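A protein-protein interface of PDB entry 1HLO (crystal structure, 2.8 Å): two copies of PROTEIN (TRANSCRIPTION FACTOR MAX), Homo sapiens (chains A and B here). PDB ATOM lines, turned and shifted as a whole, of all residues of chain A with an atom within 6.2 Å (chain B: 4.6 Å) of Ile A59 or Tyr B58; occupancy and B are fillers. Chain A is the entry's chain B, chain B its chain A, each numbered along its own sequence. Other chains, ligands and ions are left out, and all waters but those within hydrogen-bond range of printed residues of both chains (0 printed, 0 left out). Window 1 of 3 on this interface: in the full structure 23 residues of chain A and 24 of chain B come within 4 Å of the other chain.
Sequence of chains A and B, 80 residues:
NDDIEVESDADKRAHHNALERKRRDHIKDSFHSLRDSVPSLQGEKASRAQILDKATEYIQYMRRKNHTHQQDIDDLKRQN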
ATOM      1  N   LEU A  34      34.501 -31.470  33.141  1.00  0.00           N
ATOM      2  CA  LEU A  34      33.143 -30.946  32.947  1.00  0.00           C
ATOM      3  C   LEU A  34      32.807 -30.229  34.243  1.00  0.00           C
ATOM      4  O   LEU A  34      32.326 -29.112  34.219  1.00  0.00           O
ATOM      5  CB  LEU A  34      32.106 -32.056  32.739  1.00  0.00           C
ATOM      6  CG  LEU A  34      30.957 -31.841  31.751  1.00  0.00           C
ATOM      7  CD1 LEU A  34      29.790 -32.781  32.045  1.00  0.00           C
ATOM      8  CD2 LEU A  34      30.501 -30.439  31.760  1.00  0.00           C
ATOM      9  N   LYS A  54      23.551 -30.831  36.534  1.00  0.00           N
ATOM     10  CA  LYS A  54      23.814 -29.411  36.603  1.00  0.00           C
ATOM     11  C   LYS A  54      24.453 -28.920  35.307  1.00  0.00           C
ATOM     12  O   LYS A  54      24.258 -27.768  34.944  1.00  0.00           O
ATOM     13  CB  LYS A  54      24.667 -29.069  37.814  1.00  0.00           C
ATOM     14  CG  LYS A  54      23.983 -29.420  39.096  1.00  0.00           C
ATOM     15  CD  LYS A  54      24.419 -28.497  40.235  1.00  0.00           C
ATOM     16  CE  LYS A  54      23.804 -28.935  41.552  1.00  0.00           C
ATOM     17  NZ  LYS A  54      24.329 -28.187  42.732  1.00  0.00           N
ATOM     18  N   ALA A  55      25.189 -29.791  34.605  1.00  0.00           N
ATOM     19  CA  ALA A  55      25.824 -29.434  33.336  1.00  0.00           C
ATOM     20  C   ALA A  55      24.745 -29.244  32.311  1.00  0.00           C
ATOM     21  O   ALA A  55      24.721 -28.257  31.570  1.00  0.00           O
ATOM     22  CB  ALA A  55      26.752 -30.508  32.875  1.00  0.00           C
ATOM     23  N   THR A  56      23.856 -30.219  32.247  1.00  0.00           N
ATOM     24  CA  THR A  56      22.772 -30.150  31.294  1.00  0.00           C
ATOM     25  C   THR A  56      22.029 -28.846  31.464  1.00  0.00           C
ATOM     26  O   THR A  56      21.666 -28.219  30.471  1.00  0.00           O
ATOM     27  CB  THR A  56      21.766 -31.208  31.519  1.00  0.00           C
ATOM     28  OG1 THR A  56      22.358 -32.487  31.295  1.00  0.00           O
ATOM     29  CG2 THR A  56      20.507 -30.957  30.608  1.00  0.00           C
ATOM     30  N   GLU A  57      21.778 -28.479  32.731  1.00  0.00           N
ATOM     31  CA  GLU A  57      21.085 -27.239  33.111  1.00  0.00           C
ATOM     32  C   GLU A  57      21.837 -26.042  32.516  1.00  0.00           C
ATOM     33  O   GLU A  57      21.260 -25.249  31.781  1.00  0.00           O
ATOM     34  CB  GLU A  57      21.102 -27.070  34.624  1.00  0.00           C
ATOM     35  CG  GLU A  57      19.905 -27.460  35.477  1.00  0.00           C
ATOM     36  CD  GLU A  57      20.088 -27.029  36.976  1.00  0.00           C
ATOM     37  OE1 GLU A  57      21.219 -27.030  37.500  1.00  0.00           O
ATOM     38  OE2 GLU A  57      19.113 -26.685  37.660  1.00  0.00           O
ATOM     39  N   TYR A  58      23.141 -25.952  32.781  1.00  0.00           N
ATOM     40  CA  TYR A  58      24.003 -24.846  32.308  1.00  0.00           C
ATOM     41  C   TYR A  58      24.082 -24.729  30.826  1.00  0.00           C
ATOM     42  O   TYR A  58      23.969 -23.655  30.293  1.00  0.00           O
ATOM     43  CB  TYR A  58      25.399 -25.009  32.852  1.00  0.00           C
ATOM     44  CG  TYR A  58      26.412 -23.951  32.497  1.00  0.00           C
ATOM     45  CD1 TYR A  58      27.563 -24.281  31.799  1.00  0.00           C
ATOM     46  CD2 TYR A  58      26.245 -22.626  32.895  1.00  0.00           C
ATOM     47  CE1 TYR A  58      28.510 -23.314  31.492  1.00  0.00           C
ATOM     48  CE2 TYR A  58      27.190 -21.657  32.610  1.00  0.00           C
ATOM     49  CZ  TYR A  58      28.314 -22.005  31.901  1.00  0.00           C
ATOM     50  OH  TYR A  58      29.229 -21.044  31.555  1.00  0.00           O
ATOM     51  N   ILE A  59      24.269 -25.832  30.139  1.00  0.00           N
ATOM     52  CA  ILE A  59      24.344 -25.773  28.703  1.00  0.00           C
ATOM     53  C   ILE A  59      23.070 -25.200  28.105  1.00  0.00           C
ATOM     54  O   ILE A  59      23.145 -24.345  27.229  1.00  0.00           O
ATOM     55  CB  ILE A  59      24.753 -27.119  28.126  1.00  0.00           C
ATOM     56  CG1 ILE A  59      26.232 -27.342  28.505  1.00  0.00           C
ATOM     57  CG2 ILE A  59      24.671 -27.085  26.608  1.00  0.00           C
ATOM     58  CD1 ILE A  59      26.749 -28.639  28.105  1.00  0.00           C
ATOM     59  N   GLN A  60      21.915 -25.555  28.666  1.00  0.00           N
ATOM     60  CA  GLN A  60      20.623 -25.044  28.186  1.00  0.00           C
ATOM     61  C   GLN A  60      20.450 -23.560  28.455  1.00  0.00           C
ATOM     62  O   GLN A  60      19.913 -22.822  27.622  1.00  0.00           O
ATOM     63  CB  GLN A  60      19.501 -25.826  28.818  1.00  0.00           C
ATOM     64  CG  GLN A  60      19.429 -27.278  28.290  1.00  0.00           C
ATOM     65  CD  GLN A  60      18.992 -27.360  26.827  1.00  0.00           C
ATOM     66  OE1 GLN A  60      18.921 -26.356  26.115  1.00  0.00           O
ATOM     67  NE2 GLN A  60      18.727 -28.557  26.371  1.00  0.00           N
ATOM     68  N   TYR A  61      20.841 -23.152  29.654  1.00  0.00           N
ATOM     69  CA  TYR A  61      20.818 -21.764  30.072  1.00  0.00           C
ATOM     70  C   TYR A  61      21.652 -20.968  29.073  1.00  0.00           C
ATOM     71  O   TYR A  61      21.137 -20.026  28.476  1.00  0.00           O
ATOM     72  CB  TYR A  61      21.460 -21.702  31.442  1.00  0.00           C
ATOM     73  CG  TYR A  61      21.847 -20.361  31.935  1.00  0.00           C
ATOM     74  CD1 TYR A  61      23.184 -20.084  32.230  1.00  0.00           C
ATOM     75  CD2 TYR A  61      20.894 -19.399  32.188  1.00  0.00           C
ATOM     76  CE1 TYR A  61      23.569 -18.882  32.771  1.00  0.00           C
ATOM     77  CE2 TYR A  61      21.258 -18.190  32.728  1.00  0.00           C
ATOM     78  CZ  TYR A  61      22.598 -17.938  33.016  1.00  0.00           C
ATOM     79  OH  TYR A  61      22.947 -16.727  33.546  1.00  0.00           O
ATOM     80  N   MET A  62      22.921 -21.368  28.873  1.00  0.00           N
ATOM     81  CA  MET A  62      23.839 -20.702  27.934  1.00  0.00           C
ATOM     82  C   MET A  62      23.232 -20.567  26.556  1.00  0.00           C
ATOM     83  O   MET A  62      23.359 -19.520  25.925  1.00  0.00           O
ATOM     84  CB  MET A  62      25.168 -21.430  27.773  1.00  0.00           C
ATOM     85  CG  MET A  62      26.186 -21.045  28.797  1.00  0.00           C
ATOM     86  SD  MET A  62      26.091 -19.276  29.111  1.00  0.00           S
ATOM     87  CE  MET A  62      27.882 -18.853  29.232  1.00  0.00           C
ATOM     88  N   ARG A  63      22.617 -21.629  26.059  1.00  0.00           N
ATOM     89  CA  ARG A  63      22.010 -21.559  24.749  1.00  0.00           C
ATOM     90  C   ARG A  63      20.910 -20.496  24.708  1.00  0.00           C
ATOM     91  O   ARG A  63      20.845 -19.715  23.758  1.00  0.00           O
ATOM     92  CB  ARG A  63      21.495 -22.926  24.336  1.00  0.00           C
ATOM     93  CG  ARG A  63      22.570 -23.923  24.464  1.00  0.00           C
ATOM     94  CD  ARG A  63      22.125 -25.223  24.007  1.00  0.00           C
ATOM     95  NE  ARG A  63      21.743 -25.091  22.630  1.00  0.00           N
ATOM     96  CZ  ARG A  63      21.152 -26.053  21.936  1.00  0.00           C
ATOM     97  NH1 ARG A  63      20.891 -27.235  22.490  1.00  0.00           N
ATOM     98  NH2 ARG A  63      20.743 -25.804  20.705  1.00  0.00           N
ATOM     99  N   ARG A  64      20.089 -20.427  25.751  1.00  0.00           N
ATOM    100  CA  ARG A  64      19.029 -19.426  25.816  1.00  0.00           C
ATOM    101  C   ARG A  64      19.603 -18.041  25.833  1.00  0.00           C
ATOM    102  O   ARG A  64      19.300 -17.195  25.010  1.00  0.00           O
ATOM    103  CB  ARG A  64      18.231 -19.584  27.084  1.00  0.00           C
ATOM    104  CG  ARG A  64      17.128 -20.554  26.902  1.00  0.00           C
ATOM    105  CD  ARG A  64      15.847 -19.833  26.797  1.00  0.00           C
ATOM    106  NE  ARG A  64      15.943 -18.747  25.842  1.00  0.00           N
ATOM    107  CZ  ARG A  64      15.577 -18.861  24.577  1.00  0.00           C
ATOM    108  NH1 ARG A  64      15.101 -20.034  24.152  1.00  0.00           N
ATOM    109  NH2 ARG A  64      15.615 -17.787  23.781  1.00  0.00           N
ATOM    110  N   LEU B  34      22.106 -34.796  28.386  1.00  0.00           N
ATOM    111  CA  LEU B  34      23.285 -33.957  28.086  1.00  0.00           C
ATOM    112  C   LEU B  34      23.528 -34.070  26.575  1.00  0.00           C
ATOM    113  O   LEU B  34      23.698 -33.079  25.894  1.00  0.00           O
ATOM    114  CB  LEU B  34      24.548 -34.455  28.788  1.00  0.00           C
ATOM    115  CG  LEU B  34      25.545 -33.436  29.347  1.00  0.00           C
ATOM    116  CD1 LEU B  34      26.940 -34.082  29.600  1.00  0.00           C
ATOM    117  CD2 LEU B  34      25.614 -32.262  28.465  1.00  0.00           C
ATOM    118  N   SER B  37      21.337 -31.883  24.648  1.00  0.00           N
ATOM    119  CA  SER B  37      21.523 -30.463  24.924  1.00  0.00           C
ATOM    120  C   SER B  37      22.673 -29.869  24.146  1.00  0.00           C
ATOM    121  O   SER B  37      22.795 -28.641  24.038  1.00  0.00           O
ATOM    122  CB  SER B  37      21.797 -30.253  26.396  1.00  0.00           C
ATOM    123  OG  SER B  37      20.656 -30.564  27.169  1.00  0.00           O
ATOM    124  N   VAL B  38      23.514 -30.742  23.598  1.00  0.00           N
ATOM    125  CA  VAL B  38      24.705 -30.319  22.866  1.00  0.00           C
ATOM    126  C   VAL B  38      24.510 -30.525  21.387  1.00  0.00           C
ATOM    127  O   VAL B  38      24.514 -31.640  20.922  1.00  0.00           O
ATOM    128  CB  VAL B  38      25.932 -31.143  23.304  1.00  0.00           C
ATOM    129  CG1 VAL B  38      27.100 -30.751  22.502  1.00  0.00           C
ATOM    130  CG2 VAL B  38      26.224 -30.936  24.741  1.00  0.00           C
ATOM    131  N   PRO B  39      24.408 -29.449  20.616  1.00  0.00           N
ATOM    132  CA  PRO B  39      24.206 -29.573  19.178  1.00  0.00           C
ATOM    133  C   PRO B  39      25.216 -30.351  18.344  1.00  0.00           C
ATOM    134  O   PRO B  39      24.865 -30.812  17.272  1.00  0.00           O
ATOM    135  CB  PRO B  39      24.065 -28.136  18.744  1.00  0.00           C
ATOM    136  CG  PRO B  39      24.853 -27.398  19.741  1.00  0.00           C
ATOM    137  CD  PRO B  39      24.419 -28.041  21.011  1.00  0.00           C
ATOM    138  N   LYS B  54      32.681 -33.412  24.451  1.00  0.00           N
ATOM    139  CA  LYS B  54      32.098 -32.378  23.600  1.00  0.00           C
ATOM    140  C   LYS B  54      31.316 -31.392  24.430  1.00  0.00           C
ATOM    141  O   LYS B  54      31.190 -30.230  24.061  1.00  0.00           O
ATOM    142  CB  LYS B  54      31.248 -32.959  22.463  1.00  0.00           C
ATOM    143  CG  LYS B  54      32.073 -33.833  21.530  1.00  0.00           C
ATOM    144  CD  LYS B  54      31.533 -33.845  20.128  1.00  0.00           C
ATOM    145  CE  LYS B  54      32.322 -34.827  19.264  1.00  0.00           C
ATOM    146  NZ  LYS B  54      31.690 -35.031  17.921  1.00  0.00           N
ATOM    147  N   ALA B  55      30.845 -31.829  25.586  1.00  0.00           N
ATOM    148  CA  ALA B  55      30.106 -30.947  26.460  1.00  0.00           C
ATOM    149  C   ALA B  55      31.062 -29.872  26.974  1.00  0.00           C
ATOM    150  O   ALA B  55      30.680 -28.716  26.983  1.00  0.00           O
ATOM    151  CB  ALA B  55      29.488 -31.719  27.586  1.00  0.00           C
ATOM    152  N   THR B  56      32.309 -30.203  27.362  1.00  0.00           N
ATOM    153  CA  THR B  56      33.302 -29.190  27.836  1.00  0.00           C
ATOM    154  C   THR B  56      33.709 -28.260  26.712  1.00  0.00           C
ATOM    155  O   THR B  56      33.889 -27.043  26.903  1.00  0.00           O
ATOM    156  CB  THR B  56      34.522 -29.869  28.369  1.00  0.00           C
ATOM    157  OG1 THR B  56      34.089 -30.737  29.429  1.00  0.00           O
ATOM    158  CG2 THR B  56      35.484 -28.879  28.928  1.00  0.00           C
ATOM    159  N   GLU B  57      33.852 -28.864  25.541  1.00  0.00           N
ATOM    160  CA  GLU B  57      34.176 -28.150  24.333  1.00  0.00           C
ATOM    161  C   GLU B  57      33.088 -27.080  24.051  1.00  0.00           C
ATOM    162  O   GLU B  57      33.409 -25.907  23.920  1.00  0.00           O
ATOM    163  CB  GLU B  57      34.332 -29.166  23.186  1.00  0.00           C
ATOM    164  CG  GLU B  57      35.812 -29.607  23.047  1.00  0.00           C
ATOM    165  CD  GLU B  57      36.098 -31.095  23.252  1.00  0.00           C
ATOM    166  OE1 GLU B  57      36.643 -31.510  24.318  1.00  0.00           O
ATOM    167  OE2 GLU B  57      35.869 -31.840  22.287  1.00  0.00           O
ATOM    168  N   TYR B  58      31.809 -27.477  24.056  1.00  0.00           N
ATOM    169  CA  TYR B  58      30.690 -26.559  23.778  1.00  0.00           C
ATOM    170  C   TYR B  58      30.631 -25.426  24.734  1.00  0.00           C
ATOM    171  O   TYR B  58      30.417 -24.305  24.321  1.00  0.00           O
ATOM    172  CB  TYR B  58      29.348 -27.248  23.834  1.00  0.00           C
ATOM    173  CG  TYR B  58      28.228 -26.432  23.211  1.00  0.00           C
ATOM    174  CD1 TYR B  58      28.167 -26.225  21.854  1.00  0.00           C
ATOM    175  CD2 TYR B  58      27.152 -26.005  23.964  1.00  0.00           C
ATOM    176  CE1 TYR B  58      27.068 -25.651  21.273  1.00  0.00           C
ATOM    177  CE2 TYR B  58      26.036 -25.412  23.377  1.00  0.00           C
ATOM    178  CZ  TYR B  58      26.007 -25.257  22.037  1.00  0.00           C
ATOM    179  OH  TYR B  58      24.855 -24.802  21.429  1.00  0.00           O
ATOM    180  N   ILE B  59      30.758 -25.719  26.018  1.00  0.00           N
ATOM    181  CA  ILE B  59      30.737 -24.677  27.033  1.00  0.00           C
ATOM    182  C   ILE B  59      31.777 -23.600  26.721  1.00  0.00           C
ATOM    183  O   ILE B  59      31.470 -22.402  26.771  1.00  0.00           O
ATOM    184  CB  ILE B  59      30.940 -25.289  28.410  1.00  0.00           C
ATOM    185  CG1 ILE B  59      29.629 -25.892  28.914  1.00  0.00           C
ATOM    186  CG2 ILE B  59      31.558 -24.318  29.344  1.00  0.00           C
ATOM    187  CD1 ILE B  59      29.766 -26.651  30.212  1.00  0.00           C
ATOM    188  N   GLN B  60      32.967 -24.016  26.292  1.00  0.00           N
ATOM    189  CA  GLN B  60      34.045 -23.070  25.937  1.00  0.00           C
ATOM    190  C   GLN B  60      33.709 -22.265  24.703  1.00  0.00           C
ATOM    191  O   GLN B  60      34.029 -21.079  24.597  1.00  0.00           O
ATOM    192  CB  GLN B  60      35.331 -23.790  25.645  1.00  0.00           C
ATOM    193  CG  GLN B  60      35.868 -24.434  26.812  1.00  0.00           C
ATOM    194  CD  GLN B  60      35.926 -23.501  27.962  1.00  0.00           C
ATOM    195  OE1 GLN B  60      36.429 -22.368  27.860  1.00  0.00           O
ATOM    196  NE2 GLN B  60      35.409 -23.960  29.093  1.00  0.00           N
ATOM    197  N   TYR B  61      33.179 -22.958  23.716  1.00  0.00           N
ATOM    198  CA  TYR B  61      32.760 -22.333  22.491  1.00  0.00           C
ATOM    199  C   TYR B  61      31.782 -21.222  22.807  1.00  0.00           C
ATOM    200  O   TYR B  61      32.011 -20.090  22.437  1.00  0.00           O
ATOM    201  CB  TYR B  61      32.064 -23.360  21.650  1.00  0.00           C
ATOM    202  CG  TYR B  61      31.263 -22.770  20.532  1.00  0.00           C
ATOM    203  CD1 TYR B  61      29.966 -23.174  20.318  1.00  0.00           C
ATOM    204  CD2 TYR B  61      31.811 -21.863  19.664  1.00  0.00           C
ATOM    205  CE1 TYR B  61      29.231 -22.703  19.266  1.00  0.00           C
ATOM    206  CE2 TYR B  61      31.085 -21.381  18.606  1.00  0.00           C
ATOM    207  CZ  TYR B  61      29.789 -21.806  18.415  1.00  0.00           C
ATOM    208  OH  TYR B  61      29.036 -21.343  17.355  1.00  0.00           O
ATOM    209  N   MET B  62      30.702 -21.565  23.507  1.00  0.00           N
ATOM    210  CA  MET B  62      29.661 -20.616  23.925  1.00  0.00           C
ATOM    211  C   MET B  62      30.245 -19.432  24.643  1.00  0.00           C
ATOM    212  O   MET B  62      29.811 -18.309  24.430  1.00  0.00           O
ATOM    213  CB  MET B  62      28.657 -21.244  24.880  1.00  0.00           C
ATOM    214  CG  MET B  62      27.920 -22.380  24.308  1.00  0.00           C
ATOM    215  SD  MET B  62      26.306 -21.898  23.886  1.00  0.00           S
ATOM    216  CE  MET B  62      26.454 -21.630  22.105  1.00  0.00           C
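Printed residues of chain A within 4 Å of Ser B37: Thr A56 (3.5 Å), Ile A59 (3.5 Å), Gln A60 (2.9 Å) and Arg A63 (2.8 Å). Tyr B58 touches just these residues of chain A: Ile A59 and Arg A63. Of the printed residues of chain A, Ile B59 touches Tyr A58 and Ile A59. The nearest printed residue of chain A that does not touch Pro B39 is Ile A59 (5.7 Å).
Leu A34 touches Thr B56, and with the chains exchanged Thr A56 touches Leu B34. Tyr A58 touches Ile B59, and with the chains exchanged Ile A59 touches Tyr B58. Ile A59 touches Leu B34, but with the chains exchanged Leu A34 does not touch Ile B59 (4.2 Å). Ile A59 touches its own counterpart, Ile B59. Of the 13 pairs that touch across the chains among the printed residues, 6 have their exchanged pair printed and touching as well.
Among the printed residues, merely in contact across the chains: Leu A34 with Leu B34, Leu A34 with Thr B56, Thr A56 with Leu B34, Thr A56 with Ser B37, Tyr A58 with Ile B59, Ile A59 with Leu B34, Ile A59 with Ser B37, Ile A59 with Tyr B58, Ile A59 with Ile B59 and Arg A63 with Pro B39.
OG of Ser B37 sits at hydrogen-bond distance from NE2 of Gln A60 (2.9 Å). NH1 of Arg A63 lies within hydrogen-bond range of O of Ser B37 (2.8 Å). The side-chain hydroxyl (OH) of Tyr B58 sits at hydrogen-bond distance from the guanidinium group (NE) of Arg A63 (3.3 Å).
Of the 12 printed residues of chain A, 6 touch a printed residue of chain B. Printed residues of chain A that touch a printed residue of chain B: Leu A34, Thr A56, Tyr A58, Ile A59, Gln A60 and Arg A63. Hydrophobic or aromatic side chains of chain A that line the printed part of chain B: Leu A34, Tyr A58 and Ile A59. Along chain B the printed residues that touch a printed residue of chain A span positions 34 to 59.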
